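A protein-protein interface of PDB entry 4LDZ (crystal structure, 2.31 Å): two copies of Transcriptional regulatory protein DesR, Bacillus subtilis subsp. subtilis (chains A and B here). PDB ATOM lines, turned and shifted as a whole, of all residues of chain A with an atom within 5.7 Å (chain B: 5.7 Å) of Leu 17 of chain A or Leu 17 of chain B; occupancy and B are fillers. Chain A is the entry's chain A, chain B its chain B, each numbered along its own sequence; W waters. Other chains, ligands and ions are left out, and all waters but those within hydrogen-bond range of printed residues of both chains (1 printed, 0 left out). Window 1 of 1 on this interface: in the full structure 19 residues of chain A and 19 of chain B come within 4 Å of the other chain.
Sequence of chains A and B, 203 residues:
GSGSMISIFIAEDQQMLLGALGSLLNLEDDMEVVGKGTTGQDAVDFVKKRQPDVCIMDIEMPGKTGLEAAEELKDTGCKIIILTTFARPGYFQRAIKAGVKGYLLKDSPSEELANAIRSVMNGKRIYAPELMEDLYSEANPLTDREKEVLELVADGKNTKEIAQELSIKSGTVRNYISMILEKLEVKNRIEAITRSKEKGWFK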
ATOM      1  N   GLU A  12      -8.845  26.860 -12.597  1.00  0.00           N
ATOM      2  CA  GLU A  12      -8.715  26.355 -13.965  1.00  0.00           C
ATOM      3  C   GLU A  12      -7.260  26.460 -14.420  1.00  0.00           C
ATOM      4  O   GLU A  12      -6.685  27.545 -14.383  1.00  0.00           O
ATOM      5  CB  GLU A  12      -9.685  27.134 -14.894  1.00  0.00           C
ATOM      6  CG  GLU A  12      -9.536  26.852 -16.380  1.00  0.00           C
ATOM      7  CD  GLU A  12      -9.638  25.387 -16.766  1.00  0.00           C
ATOM      8  OE1 GLU A  12     -10.647  24.744 -16.397  1.00  0.00           O
ATOM      9  OE2 GLU A  12      -8.704  24.881 -17.426  1.00  0.00           O
ATOM     10  N   GLN A  14      -5.947  25.979 -17.418  1.00  0.00           N
ATOM     11  CA  GLN A  14      -5.780  26.526 -18.768  1.00  0.00           C
ATOM     12  C   GLN A  14      -6.024  28.035 -18.669  1.00  0.00           C
ATOM     13  O   GLN A  14      -7.150  28.460 -18.493  1.00  0.00           O
ATOM     14  CB  GLN A  14      -6.744  25.821 -19.724  1.00  0.00           C
ATOM     15  CG  GLN A  14      -6.427  26.044 -21.183  1.00  0.00           C
ATOM     16  CD  GLN A  14      -7.529  25.507 -22.055  1.00  0.00           C
ATOM     17  OE1 GLN A  14      -7.379  24.465 -22.684  1.00  0.00           O
ATOM     18  NE2 GLN A  14      -8.676  26.182 -22.072  1.00  0.00           N
ATOM     19  N   GLN A  15      -4.951  28.820 -18.682  1.00  0.00           N
ATOM     20  CA  GLN A  15      -4.950  30.283 -18.515  1.00  0.00           C
ATOM     21  C   GLN A  15      -5.910  31.064 -19.427  1.00  0.00           C
ATOM     22  O   GLN A  15      -6.487  32.079 -19.008  1.00  0.00           O
ATOM     23  CB  GLN A  15      -3.544  30.823 -18.652  1.00  0.00           C
ATOM     24  CG  GLN A  15      -2.923  31.207 -17.327  1.00  0.00           C
ATOM     25  CD  GLN A  15      -1.881  32.257 -17.565  1.00  0.00           C
ATOM     26  OE1 GLN A  15      -2.135  33.465 -17.449  1.00  0.00           O
ATOM     27  NE2 GLN A  15      -0.702  31.818 -17.969  1.00  0.00           N
ATOM     28  N   MET A  16      -6.070  30.599 -20.664  1.00  0.00           N
ATOM     29  CA  MET A  16      -6.997  31.195 -21.635  1.00  0.00           C
ATOM     30  C   MET A  16      -8.441  31.058 -21.117  1.00  0.00           C
ATOM     31  O   MET A  16      -9.152  32.057 -21.031  1.00  0.00           O
ATOM     32  CB  MET A  16      -6.838  30.492 -22.996  1.00  0.00           C
ATOM     33  CG  MET A  16      -7.597  31.113 -24.134  1.00  0.00           C
ATOM     34  SD  MET A  16      -6.930  32.715 -24.598  1.00  0.00           S
ATOM     35  CE  MET A  16      -5.333  32.281 -25.081  1.00  0.00           C
ATOM     36  N   LEU A  17      -8.859  29.833 -20.733  1.00  0.00           N
ATOM     37  CA  LEU A  17     -10.215  29.632 -20.235  1.00  0.00           C
ATOM     38  C   LEU A  17     -10.455  30.324 -18.910  1.00  0.00           C
ATOM     39  O   LEU A  17     -11.516  30.947 -18.747  1.00  0.00           O
ATOM     40  CB  LEU A  17     -10.596  28.158 -20.175  1.00  0.00           C
ATOM     41  CG  LEU A  17     -12.031  27.814 -19.737  1.00  0.00           C
ATOM     42  CD1 LEU A  17     -13.100  28.429 -20.679  1.00  0.00           C
ATOM     43  CD2 LEU A  17     -12.189  26.346 -19.669  1.00  0.00           C
ATOM     44  N   LEU A  18      -9.478  30.236 -17.972  1.00  0.00           N
ATOM     45  CA  LEU A  18      -9.544  30.895 -16.677  1.00  0.00           C
ATOM     46  C   LEU A  18      -9.885  32.374 -16.832  1.00  0.00           C
ATOM     47  O   LEU A  18     -10.835  32.850 -16.199  1.00  0.00           O
ATOM     48  CB  LEU A  18      -8.197  30.754 -15.924  1.00  0.00           C
ATOM     49  CG  LEU A  18      -8.108  31.389 -14.499  1.00  0.00           C
ATOM     50  CD1 LEU A  18      -9.183  30.822 -13.530  1.00  0.00           C
ATOM     51  CD2 LEU A  18      -6.751  31.179 -13.914  1.00  0.00           C
ATOM     52  N   GLY A  19      -9.123  33.068 -17.679  1.00  0.00           N
ATOM     53  CA  GLY A  19      -9.284  34.497 -17.927  1.00  0.00           C
ATOM     54  C   GLY A  19     -10.594  34.863 -18.592  1.00  0.00           C
ATOM     55  O   GLY A  19     -11.229  35.857 -18.214  1.00  0.00           O
ATOM     56  N   ALA A  20     -11.015  34.053 -19.577  1.00  0.00           N
ATOM     57  CA  ALA A  20     -12.262  34.255 -20.304  1.00  0.00           C
ATOM     58  C   ALA A  20     -13.498  33.970 -19.424  1.00  0.00           C
ATOM     59  O   ALA A  20     -14.459  34.729 -19.503  1.00  0.00           O
ATOM     60  CB  ALA A  20     -12.278  33.429 -21.576  1.00  0.00           C
ATOM     61  N   LEU A  21     -13.446  32.948 -18.541  1.00  0.00           N
ATOM     62  CA  LEU A  21     -14.496  32.658 -17.562  1.00  0.00           C
ATOM     63  C   LEU A  21     -14.612  33.784 -16.549  1.00  0.00           C
ATOM     64  O   LEU A  21     -15.716  34.147 -16.207  1.00  0.00           O
ATOM     65  CB  LEU A  21     -14.242  31.350 -16.813  1.00  0.00           C
ATOM     66  CG  LEU A  21     -14.411  30.071 -17.596  1.00  0.00           C
ATOM     67  CD1 LEU A  21     -13.985  28.873 -16.775  1.00  0.00           C
ATOM     68  CD2 LEU A  21     -15.859  29.898 -18.113  1.00  0.00           C
ATOM     69  N   GLY A  22     -13.483  34.290 -16.042  1.00  0.00           N
ATOM     70  CA  GLY A  22     -13.452  35.386 -15.079  1.00  0.00           C
ATOM     71  C   GLY A  22     -14.141  36.631 -15.592  1.00  0.00           C
ATOM     72  O   GLY A  22     -14.992  37.187 -14.903  1.00  0.00           O
ATOM     73  N   LEU A  83     -16.432  22.099 -13.283  1.00  0.00           N
ATOM     74  CA  LEU A  83     -16.543  22.482 -14.710  1.00  0.00           C
ATOM     75  C   LEU A  83     -15.375  21.792 -15.386  1.00  0.00           C
ATOM     76  O   LEU A  83     -14.240  22.170 -15.160  1.00  0.00           O
ATOM     77  CB  LEU A  83     -16.517  24.008 -14.947  1.00  0.00           C
ATOM     78  CG  LEU A  83     -16.606  24.435 -16.427  1.00  0.00           C
ATOM     79  CD1 LEU A  83     -17.905  23.942 -17.098  1.00  0.00           C
ATOM     80  CD2 LEU A  83     -16.469  25.926 -16.562  1.00  0.00           C
ATOM     81  N   LYS A 106     -17.580  21.151 -20.160  1.00  0.00           N
ATOM     82  CA  LYS A 106     -17.056  22.244 -20.976  1.00  0.00           C
ATOM     83  C   LYS A 106     -17.659  22.267 -22.387  1.00  0.00           C
ATOM     84  O   LYS A 106     -17.497  23.225 -23.135  1.00  0.00           O
ATOM     85  CB  LYS A 106     -15.520  22.252 -20.969  1.00  0.00           C
ATOM     86  CG  LYS A 106     -14.915  22.782 -19.647  1.00  0.00           C
ATOM     87  CD  LYS A 106     -13.375  22.664 -19.647  1.00  0.00           C
ATOM     88  CE  LYS A 106     -12.772  23.168 -18.364  1.00  0.00           C
ATOM     89  NZ  LYS A 106     -11.320  22.886 -18.290  1.00  0.00           N
ATOM     90  N   GLU B  12     -13.852  26.367 -32.498  1.00  0.00           N
ATOM     91  CA  GLU B  12     -13.479  25.724 -31.233  1.00  0.00           C
ATOM     92  C   GLU B  12     -14.561  24.707 -30.847  1.00  0.00           C
ATOM     93  O   GLU B  12     -15.733  25.072 -30.755  1.00  0.00           O
ATOM     94  CB  GLU B  12     -13.261  26.813 -30.147  1.00  0.00           C
ATOM     95  CG  GLU B  12     -13.079  26.302 -28.725  1.00  0.00           C
ATOM     96  CD  GLU B  12     -11.951  25.311 -28.573  1.00  0.00           C
ATOM     97  OE1 GLU B  12     -10.821  25.619 -29.015  1.00  0.00           O
ATOM     98  OE2 GLU B  12     -12.211  24.203 -28.052  1.00  0.00           O
ATOM     99  N   GLN B  14     -14.920  22.998 -28.032  1.00  0.00           N
ATOM    100  CA  GLN B  14     -15.330  23.080 -26.633  1.00  0.00           C
ATOM    101  C   GLN B  14     -16.219  24.313 -26.507  1.00  0.00           C
ATOM    102  O   GLN B  14     -15.728  25.439 -26.541  1.00  0.00           O
ATOM    103  CB  GLN B  14     -14.087  23.142 -25.749  1.00  0.00           C
ATOM    104  CG  GLN B  14     -14.335  22.838 -24.307  1.00  0.00           C
ATOM    105  CD  GLN B  14     -13.094  23.102 -23.499  1.00  0.00           C
ATOM    106  OE1 GLN B  14     -12.363  22.177 -23.122  1.00  0.00           O
ATOM    107  NE2 GLN B  14     -12.798  24.370 -23.258  1.00  0.00           N
ATOM    108  N   GLN B  15     -17.535  24.098 -26.449  1.00  0.00           N
ATOM    109  CA  GLN B  15     -18.562  25.149 -26.397  1.00  0.00           C
ATOM    110  C   GLN B  15     -18.361  26.219 -25.316  1.00  0.00           C
ATOM    111  O   GLN B  15     -18.703  27.386 -25.531  1.00  0.00           O
ATOM    112  CB  GLN B  15     -19.933  24.506 -26.258  1.00  0.00           C
ATOM    113  CG  GLN B  15     -20.750  24.481 -27.523  1.00  0.00           C
ATOM    114  CD  GLN B  15     -22.208  24.649 -27.185  1.00  0.00           C
ATOM    115  OE1 GLN B  15     -22.775  25.748 -27.334  1.00  0.00           O
ATOM    116  NE2 GLN B  15     -22.814  23.603 -26.619  1.00  0.00           N
ATOM    117  N   MET B  16     -17.846  25.816 -24.157  1.00  0.00           N
ATOM    118  CA  MET B  16     -17.559  26.723 -23.051  1.00  0.00           C
ATOM    119  C   MET B  16     -16.473  27.709 -23.473  1.00  0.00           C
ATOM    120  O   MET B  16     -16.685  28.907 -23.346  1.00  0.00           O
ATOM    121  CB  MET B  16     -17.127  25.934 -21.790  1.00  0.00           C
ATOM    122  CG  MET B  16     -17.044  26.777 -20.528  1.00  0.00           C
ATOM    123  SD  MET B  16     -18.599  27.537 -20.008  1.00  0.00           S
ATOM    124  CE  MET B  16     -19.676  26.075 -19.804  1.00  0.00           C
ATOM    125  N   LEU B  17     -15.330  27.224 -23.998  1.00  0.00           N
ATOM    126  CA  LEU B  17     -14.261  28.128 -24.416  1.00  0.00           C
ATOM    127  C   LEU B  17     -14.670  28.992 -25.595  1.00  0.00           C
ATOM    128  O   LEU B  17     -14.416  30.189 -25.554  1.00  0.00           O
ATOM    129  CB  LEU B  17     -12.960  27.388 -24.694  1.00  0.00           C
ATOM    130  CG  LEU B  17     -11.751  28.232 -25.108  1.00  0.00           C
ATOM    131  CD1 LEU B  17     -11.356  29.274 -24.021  1.00  0.00           C
ATOM    132  CD2 LEU B  17     -10.594  27.332 -25.416  1.00  0.00           C
ATOM    133  N   LEU B  18     -15.327  28.399 -26.614  1.00  0.00           N
ATOM    134  CA  LEU B  18     -15.850  29.104 -27.782  1.00  0.00           C
ATOM    135  C   LEU B  18     -16.650  30.345 -27.351  1.00  0.00           C
ATOM    136  O   LEU B  18     -16.367  31.441 -27.820  1.00  0.00           O
ATOM    137  CB  LEU B  18     -16.770  28.162 -28.619  1.00  0.00           C
ATOM    138  CG  LEU B  18     -17.386  28.750 -29.920  1.00  0.00           C
ATOM    139  CD1 LEU B  18     -16.310  29.226 -30.892  1.00  0.00           C
ATOM    140  CD2 LEU B  18     -18.266  27.729 -30.607  1.00  0.00           C
ATOM    141  N   GLY B  19     -17.631  30.152 -26.467  1.00  0.00           N
ATOM    142  CA  GLY B  19     -18.500  31.218 -25.992  1.00  0.00           C
ATOM    143  C   GLY B  19     -17.815  32.267 -25.162  1.00  0.00           C
ATOM    144  O   GLY B  19     -18.087  33.456 -25.321  1.00  0.00           O
ATOM    145  N   ALA B  20     -16.924  31.831 -24.266  1.00  0.00           N
ATOM    146  CA  ALA B  20     -16.172  32.720 -23.392  1.00  0.00           C
ATOM    147  C   ALA B  20     -15.096  33.532 -24.173  1.00  0.00           C
ATOM    148  O   ALA B  20     -14.890  34.712 -23.869  1.00  0.00           O
ATOM    149  CB  ALA B  20     -15.556  31.918 -22.253  1.00  0.00           C
ATOM    150  N   LEU B  21     -14.457  32.928 -25.189  1.00  0.00           N
ATOM    151  CA  LEU B  21     -13.486  33.610 -26.062  1.00  0.00           C
ATOM    152  C   LEU B  21     -14.197  34.678 -26.894  1.00  0.00           C
ATOM    153  O   LEU B  21     -13.656  35.787 -27.037  1.00  0.00           O
ATOM    154  CB  LEU B  21     -12.771  32.644 -27.039  1.00  0.00           C
ATOM    155  CG  LEU B  21     -11.477  31.963 -26.575  1.00  0.00           C
ATOM    156  CD1 LEU B  21     -10.881  31.129 -27.711  1.00  0.00           C
ATOM    157  CD2 LEU B  21     -10.441  32.974 -26.018  1.00  0.00           C
ATOM    158  N   GLY B  22     -15.375  34.310 -27.449  1.00  0.00           N
ATOM    159  CA  GLY B  22     -16.220  35.200 -28.233  1.00  0.00           C
ATOM    160  C   GLY B  22     -16.553  36.449 -27.443  1.00  0.00           C
ATOM    161  O   GLY B  22     -16.360  37.555 -27.947  1.00  0.00           O
ATOM    162  N   LEU B  83      -5.157  28.390 -32.269  1.00  0.00           N
ATOM    163  CA  LEU B  83      -5.217  28.525 -30.799  1.00  0.00           C
ATOM    164  C   LEU B  83      -5.509  27.115 -30.301  1.00  0.00           C
ATOM    165  O   LEU B  83      -6.600  26.598 -30.524  1.00  0.00           O
ATOM    166  CB  LEU B  83      -6.292  29.517 -30.316  1.00  0.00           C
ATOM    167  CG  LEU B  83      -6.398  29.685 -28.794  1.00  0.00           C
ATOM    168  CD1 LEU B  83      -5.109  30.216 -28.201  1.00  0.00           C
ATOM    169  CD2 LEU B  83      -7.554  30.558 -28.424  1.00  0.00           C
ATOM    170  N   LYS B 106      -3.237  27.656 -25.647  1.00  0.00           N
ATOM    171  CA  LYS B 106      -4.338  27.955 -24.734  1.00  0.00           C
ATOM    172  C   LYS B 106      -3.835  28.168 -23.284  1.00  0.00           C
ATOM    173  O   LYS B 106      -4.540  28.724 -22.444  1.00  0.00           O
ATOM    174  CB  LYS B 106      -5.387  26.841 -24.797  1.00  0.00           C
ATOM    175  CG  LYS B 106      -6.371  27.006 -25.924  1.00  0.00           C
ATOM    176  CD  LYS B 106      -7.257  25.769 -26.046  1.00  0.00           C
ATOM    177  CE  LYS B 106      -8.029  25.801 -27.352  1.00  0.00           C
ATOM    178  NZ  LYS B 106      -8.721  24.516 -27.630  1.00  0.00           N
HETATM  179  O   HOH W   1     -15.694  36.124 -21.568  1.00  0.00           O
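Of the 12 printed residues of chain B, 8 touch a printed residue of chain A. Hydrophobic or aromatic side chains of chain B within 4 Å of the printed part of chain A: Met 16, Leu 17, Ala 20, Leu 21 and Leu 83. Printed residues of chain A that touch a printed residue of chain B: Gln 14, Gln 15, Met 16, Leu 17, Ala 20, Leu 83 and Lys 106. Hydrophobic or aromatic side chains of chain A within 4 Å of the printed part of chain B: Met 16, Leu 17, Ala 20 and Leu 83. Among the printed residues, no Asp or Glu carboxylate lies within 4 Å of a Lys or Arg side-chain nitrogen of the other chain.
N of Met 16 of chain A lies close to O of Lys 106 of chain B (3.0 Å). The backbone carbonyl oxygen (O) of Lys 106 of chain A lies within hydrogen-bond range of the backbone NH (N) of Gln 15 of chain B (3.4 Å). O of Lys 106 of chain A is in hydrogen-bond range of N of Met 16 of chain B, 2.8 Å away.
Gln 14 of chain A touches Lys 106 of chain B. Lys 106 of chain B touches Gln 15 of chain A. Met 16 of chain A touches Leu 21 of chain B. Met 16 of chain A touches Leu 83 of chain B. Leu 17 of chain B touches Leu 17 of chain A. Ala 20 of chain A touches Ala 20 of chain B. Leu 83 of chain A touches Met 16 of chain B. Lys 106 of chain A touches Gln 14 of chain B (O to CG, 3.4 Å).
Of the printed residues of chain B, Leu 17 of chain A touches Leu 17. Leu 17 of chain B touches just one residue of chain A: Leu 17. Printed residues of chain A within 4 Å of Met 16 of chain B: Leu 83 and Lys 106. Printed residues of chain A within 4 Å of Leu 21 of chain B: Met 16. Printed residues of chain B within 4 Å of Lys 106 of chain A: Gln 14 (3.4 Å), Gln 15 (3.4 Å) and Met 16 (2.8 Å). Printed residues of chain B within 4 Å of Gln 14 of chain A: Lys 106. Of the printed residues of chain A, Lys 106 of chain B touches Gln 14, Gln 15 and Met 16. The nearest printed residue of chain A that does not touch Leu 83 of chain B is Gln 14 of chain A (7.8 Å).
Water W1 lies within hydrogen-bond range of O of Ala 20 of chain A and O of Ala 20 of chain B.
Gln 14 of chain A touches Lys 106 of chain B, and with the chains exchanged Lys 106 of chain A touches Gln 14 of chain B. Gln 15 of chain A touches Lys 106 of chain B, and with the chains exchanged Lys 106 of chain A touches Gln 15 of chain B. Met 16 of chain A touches Leu 83 of chain B, and with the chains exchanged Leu 83 of chain A touches Met 16 of chain B. Leu 17 of chain A touches its own counterpart, Leu 17 of chain B. Of the 11 pairs that touch across the chains among the printed residues, 10 have their exchanged pair printed and touching as well.
The side-chain carboxylate of Glu 12 of chain A is in hydrogen-bond range of the backbone NH of Gln 14 of chain A, 3.0 Å away. OE1 of Glu 12 of chain A lies within salt-bridge range of NZ of Lys 106 of chain A (2.7 Å). The side-chain carboxylate of Glu 12 of chain B sits at hydrogen-bond distance from the backbone NH of Gln 14 of chain B, at 3.0 Å. NZ of Lys 106 of chain B is in salt-bridge range of OE1 of Glu 12 of chain B (2.7 Å).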
